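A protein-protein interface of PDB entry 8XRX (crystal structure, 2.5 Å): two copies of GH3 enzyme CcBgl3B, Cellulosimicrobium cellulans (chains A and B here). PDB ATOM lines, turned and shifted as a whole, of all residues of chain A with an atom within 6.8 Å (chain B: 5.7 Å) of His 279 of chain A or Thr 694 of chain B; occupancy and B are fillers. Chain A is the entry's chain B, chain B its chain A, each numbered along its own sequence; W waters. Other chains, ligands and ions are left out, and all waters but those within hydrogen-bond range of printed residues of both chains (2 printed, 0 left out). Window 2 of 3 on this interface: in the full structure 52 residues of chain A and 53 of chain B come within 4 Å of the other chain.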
ATOM      1  N   ARG A 273      -7.559  17.839 -16.136  1.00  0.00           N
ATOM      2  CA  ARG A 273      -7.018  16.699 -15.394  1.00  0.00           C
ATOM      3  C   ARG A 273      -8.010  15.544 -15.328  1.00  0.00           C
ATOM      4  O   ARG A 273      -7.602  14.382 -15.300  1.00  0.00           O
ATOM      5  CB  ARG A 273      -6.574  17.134 -13.988  1.00  0.00           C
ATOM      6  CG  ARG A 273      -5.424  18.112 -14.044  1.00  0.00           C
ATOM      7  CD  ARG A 273      -5.053  18.834 -12.755  1.00  0.00           C
ATOM      8  NE  ARG A 273      -3.667  18.488 -12.505  1.00  0.00           N
ATOM      9  CZ  ARG A 273      -2.646  19.323 -12.417  1.00  0.00           C
ATOM     10  NH1 ARG A 273      -1.442  18.825 -12.239  1.00  0.00           N
ATOM     11  NH2 ARG A 273      -2.812  20.619 -12.461  1.00  0.00           N
ATOM     12  N   MET A 274      -9.306  15.833 -15.336  1.00  0.00           N
ATOM     13  CA  MET A 274     -10.283  14.764 -15.436  1.00  0.00           C
ATOM     14  C   MET A 274     -10.132  13.956 -16.717  1.00  0.00           C
ATOM     15  O   MET A 274     -10.703  12.869 -16.822  1.00  0.00           O
ATOM     16  CB  MET A 274     -11.696  15.332 -15.357  1.00  0.00           C
ATOM     17  CG  MET A 274     -12.029  16.030 -14.061  1.00  0.00           C
ATOM     18  SD  MET A 274     -13.776  16.398 -13.814  1.00  0.00           S
ATOM     19  CE  MET A 274     -14.120  17.548 -15.138  1.00  0.00           C
ATOM     20  N   VAL A 275      -9.399  14.459 -17.705  1.00  0.00           N
ATOM     21  CA  VAL A 275      -9.184  13.709 -18.932  1.00  0.00           C
ATOM     22  C   VAL A 275      -7.842  13.006 -18.824  1.00  0.00           C
ATOM     23  O   VAL A 275      -7.779  11.775 -18.831  1.00  0.00           O
ATOM     24  CB  VAL A 275      -9.244  14.615 -20.182  1.00  0.00           C
ATOM     25  CG1 VAL A 275      -8.915  13.830 -21.449  1.00  0.00           C
ATOM     26  CG2 VAL A 275     -10.603  15.262 -20.318  1.00  0.00           C
ATOM     27  N   TRP A 276      -6.767  13.776 -18.685  1.00  0.00           N
ATOM     28  CA  TRP A 276      -5.431  13.234 -18.856  1.00  0.00           C
ATOM     29  C   TRP A 276      -4.774  12.730 -17.563  1.00  0.00           C
ATOM     30  O   TRP A 276      -3.747  12.065 -17.640  1.00  0.00           O
ATOM     31  CB  TRP A 276      -4.533  14.279 -19.552  1.00  0.00           C
ATOM     32  CG  TRP A 276      -4.274  15.535 -18.767  1.00  0.00           C
ATOM     33  CD1 TRP A 276      -4.945  16.712 -18.860  1.00  0.00           C
ATOM     34  CD2 TRP A 276      -3.248  15.741 -17.793  1.00  0.00           C
ATOM     35  NE1 TRP A 276      -4.415  17.636 -18.003  1.00  0.00           N
ATOM     36  CE2 TRP A 276      -3.375  17.059 -17.325  1.00  0.00           C
ATOM     37  CE3 TRP A 276      -2.240  14.932 -17.263  1.00  0.00           C
ATOM     38  CZ2 TRP A 276      -2.537  17.587 -16.347  1.00  0.00           C
ATOM     39  CZ3 TRP A 276      -1.410  15.460 -16.294  1.00  0.00           C
ATOM     40  CH2 TRP A 276      -1.563  16.771 -15.849  1.00  0.00           C
ATOM     41  N   GLU A 277      -5.327  12.986 -16.382  1.00  0.00           N
ATOM     42  CA  GLU A 277      -4.639  12.557 -15.168  1.00  0.00           C
ATOM     43  C   GLU A 277      -5.497  11.683 -14.261  1.00  0.00           C
ATOM     44  O   GLU A 277      -4.989  10.769 -13.623  1.00  0.00           O
ATOM     45  CB  GLU A 277      -4.142  13.769 -14.393  1.00  0.00           C
ATOM     46  CG  GLU A 277      -2.990  13.466 -13.469  1.00  0.00           C
ATOM     47  CD  GLU A 277      -2.398  14.717 -12.897  1.00  0.00           C
ATOM     48  OE1 GLU A 277      -3.184  15.657 -12.632  1.00  0.00           O
ATOM     49  OE2 GLU A 277      -1.163  14.773 -12.723  1.00  0.00           O
ATOM     50  N   GLN A 278      -6.792  11.944 -14.181  1.00  0.00           N
ATOM     51  CA  GLN A 278      -7.674  11.097 -13.403  1.00  0.00           C
ATOM     52  C   GLN A 278      -8.408  10.074 -14.258  1.00  0.00           C
ATOM     53  O   GLN A 278      -8.919   9.091 -13.720  1.00  0.00           O
ATOM     54  CB  GLN A 278      -8.671  11.964 -12.622  1.00  0.00           C
ATOM     55  CG  GLN A 278      -8.021  12.781 -11.517  1.00  0.00           C
ATOM     56  CD  GLN A 278      -8.813  14.005 -11.098  1.00  0.00           C
ATOM     57  OE1 GLN A 278      -9.446  14.645 -11.908  1.00  0.00           O
ATOM     58  NE2 GLN A 278      -8.755  14.346  -9.829  1.00  0.00           N
ATOM     59  N   HIS A 279      -8.471  10.290 -15.568  1.00  0.00           N
ATOM     60  CA  HIS A 279      -9.046   9.340 -16.524  1.00  0.00           C
ATOM     61  C   HIS A 279     -10.518   9.032 -16.249  1.00  0.00           C
ATOM     62  O   HIS A 279     -10.975   7.904 -16.409  1.00  0.00           O
ATOM     63  CB  HIS A 279      -8.194   8.071 -16.580  1.00  0.00           C
ATOM     64  CG  HIS A 279      -6.827   8.328 -17.131  1.00  0.00           C
ATOM     65  ND1 HIS A 279      -5.762   8.684 -16.338  1.00  0.00           N
ATOM     66  CD2 HIS A 279      -6.378   8.377 -18.404  1.00  0.00           C
ATOM     67  CE1 HIS A 279      -4.706   8.906 -17.094  1.00  0.00           C
ATOM     68  NE2 HIS A 279      -5.053   8.726 -18.351  1.00  0.00           N
ATOM     69  N   ILE A 280     -11.281  10.056 -15.869  1.00  0.00           N
ATOM     70  CA  ILE A 280     -12.720   9.929 -15.707  1.00  0.00           C
ATOM     71  C   ILE A 280     -13.509  10.604 -16.821  1.00  0.00           C
ATOM     72  O   ILE A 280     -14.742  10.547 -16.800  1.00  0.00           O
ATOM     73  CB  ILE A 280     -13.197  10.450 -14.341  1.00  0.00           C
ATOM     74  CG1 ILE A 280     -12.891  11.931 -14.184  1.00  0.00           C
ATOM     75  CG2 ILE A 280     -12.606   9.638 -13.217  1.00  0.00           C
ATOM     76  CD1 ILE A 280     -13.550  12.502 -12.995  1.00  0.00           C
ATOM     77  N   GLN A 281     -12.853  11.230 -17.793  1.00  0.00           N
ATOM     78  CA  GLN A 281     -13.555  11.786 -18.927  1.00  0.00           C
ATOM     79  C   GLN A 281     -12.845  11.392 -20.217  1.00  0.00           C
ATOM     80  O   GLN A 281     -11.623  11.534 -20.320  1.00  0.00           O
ATOM     81  CB  GLN A 281     -13.662  13.310 -18.808  1.00  0.00           C
ATOM     82  CG  GLN A 281     -14.562  13.788 -17.669  1.00  0.00           C
ATOM     83  CD  GLN A 281     -16.021  13.586 -17.978  1.00  0.00           C
ATOM     84  OE1 GLN A 281     -16.381  13.262 -19.096  1.00  0.00           O
ATOM     85  NE2 GLN A 281     -16.864  13.767 -16.991  1.00  0.00           N
ATOM     86  N   PRO A 282     -13.576  10.916 -21.224  1.00  0.00           N
ATOM     87  CA  PRO A 282     -12.937  10.539 -22.494  1.00  0.00           C
ATOM     88  C   PRO A 282     -12.321  11.689 -23.271  1.00  0.00           C
ATOM     89  O   PRO A 282     -11.337  11.461 -23.974  1.00  0.00           O
ATOM     90  CB  PRO A 282     -14.086   9.905 -23.282  1.00  0.00           C
ATOM     91  CG  PRO A 282     -15.305  10.489 -22.700  1.00  0.00           C
ATOM     92  CD  PRO A 282     -15.019  10.643 -21.233  1.00  0.00           C
ATOM     93  N   ARG B 624      -5.591   6.081  -9.626  1.00  0.00           N
ATOM     94  CA  ARG B 624      -4.980   7.116 -10.448  1.00  0.00           C
ATOM     95  C   ARG B 624      -5.199   8.499  -9.855  1.00  0.00           C
ATOM     96  O   ARG B 624      -6.124   8.730  -9.083  1.00  0.00           O
ATOM     97  CB  ARG B 624      -5.569   7.101 -11.850  1.00  0.00           C
ATOM     98  CG  ARG B 624      -5.240   5.904 -12.680  1.00  0.00           C
ATOM     99  CD  ARG B 624      -6.477   5.493 -13.398  1.00  0.00           C
ATOM    100  NE  ARG B 624      -6.250   4.617 -14.531  1.00  0.00           N
ATOM    101  CZ  ARG B 624      -7.216   3.875 -15.048  1.00  0.00           C
ATOM    102  NH1 ARG B 624      -8.405   3.923 -14.513  1.00  0.00           N
ATOM    103  NH2 ARG B 624      -7.001   3.075 -16.068  1.00  0.00           N
ATOM    104  N   SER B 692      -7.006  -3.367 -17.033  1.00  0.00           N
ATOM    105  CA  SER B 692      -6.997  -1.928 -16.824  1.00  0.00           C
ATOM    106  C   SER B 692      -8.207  -1.340 -17.530  1.00  0.00           C
ATOM    107  O   SER B 692      -8.394  -1.558 -18.729  1.00  0.00           O
ATOM    108  CB  SER B 692      -5.711  -1.308 -17.364  1.00  0.00           C
ATOM    109  OG  SER B 692      -5.696   0.070 -17.102  1.00  0.00           O
ATOM    110  N   ASP B 693      -9.027  -0.615 -16.788  1.00  0.00           N
ATOM    111  CA  ASP B 693     -10.179   0.078 -17.339  1.00  0.00           C
ATOM    112  C   ASP B 693      -9.719   1.480 -17.716  1.00  0.00           C
ATOM    113  O   ASP B 693      -9.297   2.246 -16.853  1.00  0.00           O
ATOM    114  CB  ASP B 693     -11.310   0.090 -16.310  1.00  0.00           C
ATOM    115  CG  ASP B 693     -12.610   0.564 -16.873  1.00  0.00           C
ATOM    116  OD1 ASP B 693     -12.588   1.297 -17.868  1.00  0.00           O
ATOM    117  OD2 ASP B 693     -13.662   0.212 -16.309  1.00  0.00           O
ATOM    118  N   THR B 694      -9.778   1.803 -19.008  1.00  0.00           N
ATOM    119  CA  THR B 694      -9.059   2.963 -19.524  1.00  0.00           C
ATOM    120  C   THR B 694      -9.695   4.283 -19.090  1.00  0.00           C
ATOM    121  O   THR B 694      -8.994   5.210 -18.681  1.00  0.00           O
ATOM    122  CB  THR B 694      -8.978   2.876 -21.041  1.00  0.00           C
ATOM    123  OG1 THR B 694      -8.337   1.652 -21.402  1.00  0.00           O
ATOM    124  CG2 THR B 694      -8.153   4.012 -21.581  1.00  0.00           C
ATOM    125  N   VAL B 695     -11.017   4.396 -19.201  1.00  0.00           N
ATOM    126  CA  VAL B 695     -11.767   5.569 -18.768  1.00  0.00           C
ATOM    127  C   VAL B 695     -12.880   5.088 -17.851  1.00  0.00           C
ATOM    128  O   VAL B 695     -13.645   4.194 -18.222  1.00  0.00           O
ATOM    129  CB  VAL B 695     -12.352   6.364 -19.962  1.00  0.00           C
ATOM    130  CG1 VAL B 695     -13.055   7.602 -19.474  1.00  0.00           C
ATOM    131  CG2 VAL B 695     -11.288   6.756 -20.908  1.00  0.00           C
ATOM    132  N   THR B 696     -12.952   5.656 -16.650  1.00  0.00           N
ATOM    133  CA  THR B 696     -13.872   5.193 -15.619  1.00  0.00           C
ATOM    134  C   THR B 696     -14.741   6.355 -15.154  1.00  0.00           C
ATOM    135  O   THR B 696     -14.322   7.504 -15.194  1.00  0.00           O
ATOM    136  CB  THR B 696     -13.114   4.549 -14.416  1.00  0.00           C
ATOM    137  OG1 THR B 696     -12.283   5.511 -13.755  1.00  0.00           O
ATOM    138  CG2 THR B 696     -12.238   3.407 -14.878  1.00  0.00           C
ATOM    139  N   SER B 697     -15.972   6.054 -14.735  1.00  0.00           N
ATOM    140  CA  SER B 697     -16.860   7.122 -14.274  1.00  0.00           C
ATOM    141  C   SER B 697     -16.380   7.733 -12.968  1.00  0.00           C
ATOM    142  O   SER B 697     -16.695   8.890 -12.680  1.00  0.00           O
ATOM    143  CB  SER B 697     -18.278   6.605 -14.104  1.00  0.00           C
ATOM    144  OG  SER B 697     -18.312   5.622 -13.092  1.00  0.00           O
ATOM    145  N   VAL B 698     -15.632   6.974 -12.170  1.00  0.00           N
ATOM    146  CA  VAL B 698     -14.981   7.459 -10.963  1.00  0.00           C
ATOM    147  C   VAL B 698     -13.540   6.992 -11.005  1.00  0.00           C
ATOM    148  O   VAL B 698     -13.198   6.060 -11.728  1.00  0.00           O
ATOM    149  CB  VAL B 698     -15.682   6.972  -9.690  1.00  0.00           C
ATOM    150  CG1 VAL B 698     -16.935   7.788  -9.467  1.00  0.00           C
ATOM    151  CG2 VAL B 698     -16.043   5.521  -9.833  1.00  0.00           C
ATOM    152  N   GLU B 745     -13.353   1.113 -23.283  1.00  0.00           N
ATOM    153  CA  GLU B 745     -12.105   0.476 -23.653  1.00  0.00           C
ATOM    154  C   GLU B 745     -11.381  -0.084 -22.434  1.00  0.00           C
ATOM    155  O   GLU B 745     -11.370   0.525 -21.364  1.00  0.00           O
ATOM    156  CB  GLU B 745     -11.199   1.468 -24.376  1.00  0.00           C
ATOM    157  CG  GLU B 745     -11.379   1.490 -25.869  1.00  0.00           C
ATOM    158  CD  GLU B 745     -10.045   1.508 -26.589  1.00  0.00           C
ATOM    159  OE1 GLU B 745      -9.872   0.731 -27.556  1.00  0.00           O
ATOM    160  OE2 GLU B 745      -9.158   2.288 -26.168  1.00  0.00           O
ATOM    161  N   PHE B 746     -10.749  -1.238 -22.620  1.00  0.00           N
ATOM    162  CA  PHE B 746      -9.967  -1.897 -21.595  1.00  0.00           C
ATOM    163  C   PHE B 746      -8.597  -2.254 -22.141  1.00  0.00           C
ATOM    164  O   PHE B 746      -8.312  -2.109 -23.330  1.00  0.00           O
ATOM    165  CB  PHE B 746     -10.654  -3.157 -21.088  1.00  0.00           C
ATOM    166  CG  PHE B 746     -11.905  -2.896 -20.300  1.00  0.00           C
ATOM    167  CD1 PHE B 746     -13.118  -2.751 -20.932  1.00  0.00           C
ATOM    168  CD2 PHE B 746     -11.869  -2.834 -18.924  1.00  0.00           C
ATOM    169  CE1 PHE B 746     -14.255  -2.532 -20.208  1.00  0.00           C
ATOM    170  CE2 PHE B 746     -12.998  -2.622 -18.207  1.00  0.00           C
ATOM    171  CZ  PHE B 746     -14.191  -2.473 -18.845  1.00  0.00           C
ATOM    172  N   GLU B 747      -7.738  -2.722 -21.244  1.00  0.00           N
ATOM    173  CA  GLU B 747      -6.429  -3.232 -21.624  1.00  0.00           C
ATOM    174  C   GLU B 747      -6.166  -4.498 -20.836  1.00  0.00           C
ATOM    175  O   GLU B 747      -6.399  -4.532 -19.629  1.00  0.00           O
ATOM    176  CB  GLU B 747      -5.334  -2.207 -21.362  1.00  0.00           C
ATOM    177  CG  GLU B 747      -4.286  -2.132 -22.433  1.00  0.00           C
ATOM    178  CD  GLU B 747      -3.236  -1.081 -22.135  1.00  0.00           C
ATOM    179  OE1 GLU B 747      -3.027  -0.772 -20.945  1.00  0.00           O
ATOM    180  OE2 GLU B 747      -2.603  -0.575 -23.084  1.00  0.00           O
HETATM  181  O   HOH W   1     -16.711  10.459 -14.932  1.00  0.00           O
HETATM  182  O   HOH W   2      -9.657   6.398 -13.124  1.00  0.00           O
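His 279 of chain A touches three residues of chain B.
Of chain A, only His 279 (3.6 Å) comes within 4 Å of Thr 694 of chain B.
Printed residues of chain B within 4 Å of Ile 280 of chain A: Thr 696 and Val 698.
Of the printed residues of chain B, Pro 282 of chain A touches Val 695.
Printed residues of chain A within 4 Å of Thr 696 of chain B: His 279 and Ile 280.
Printed residues of chain A within 4 Å of Val 695 of chain B: His 279 (3.4 Å), Gln 281 (3.9 Å) and Pro 282 (3.8 Å).
Of the printed residues of chain A, Val 698 of chain B touches Ile 280 (3.6 Å).
Glu 745 of chain B touches none of the printed residues of chain A.
The nearest printed residue of chain B that does not touch Ile 280 of chain A is Val 695 of chain B (4.03 Å).
No position is printed for both chains.
Of the 7 pairs that touch across the chains among the printed residues, none has its exchanged pair printed and touching as well.
Hydrophobic or aromatic side chains of chain A within 4 Å of the printed part of chain B: His 279 and Ile 280.
Of the 11 printed residues of chain B, 4 touch a printed residue of chain A.
Printed residues of chain B that touch a printed residue of chain A: Thr 694, Val 695, Thr 696 and Val 698.
Hydrophobic or aromatic side chains of chain B that line the printed part of chain A: Val 695.
The backbone carbonyl oxygen (O) of Glu 745 of chain B is in hydrogen-bond range of the backbone NH (N) of Thr 694 of chain B.
The backbone carbonyl oxygen (O) of Met 274 of chain A sits at hydrogen-bond distance from the backbone NH (N) of Ile 280 of chain A, at 3.0 Å.
The backbone carbonyl oxygen (O) of Met 274 of chain A sits at hydrogen-bond distance from the backbone NH (N) of Gln 281 of chain A (2.9 Å).
N of Thr 696 of chain B sits at hydrogen-bond distance from O of His 279 of chain A (3.0 Å).
The backbone carbonyl oxygen (O) of Ile 280 of chain A lies close to the backbone carbonyl oxygen (O) of Thr 696 of chain B (3.5 Å).
Water W1 lies within hydrogen-bond range of O of Ile 280 of chain A (2.7 Å) and O of Ser 697 of chain B (2.7 Å).
Water W2 lies within hydrogen-bond range of OG1 of Thr 696 of chain B (2.8 Å), O of Gln 278 of chain A (2.9 Å) and NH1 of Arg 624 of chain B (3.1 Å).
His 279 of chain A touches Thr 694 of chain B (CB to O, 3.6 Å).
His 279 of chain A touches Val 695 of chain B (O to CA, 3.4 Å).
C of Val 698 of chain B touches CG2 of Ile 280 of chain A, at 3.6 Å.
CG1 of Val 695 of chain B touches C of Gln 281 of chain A, 3.9 Å away.
Val 695 of chain B touches Pro 282 of chain A.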
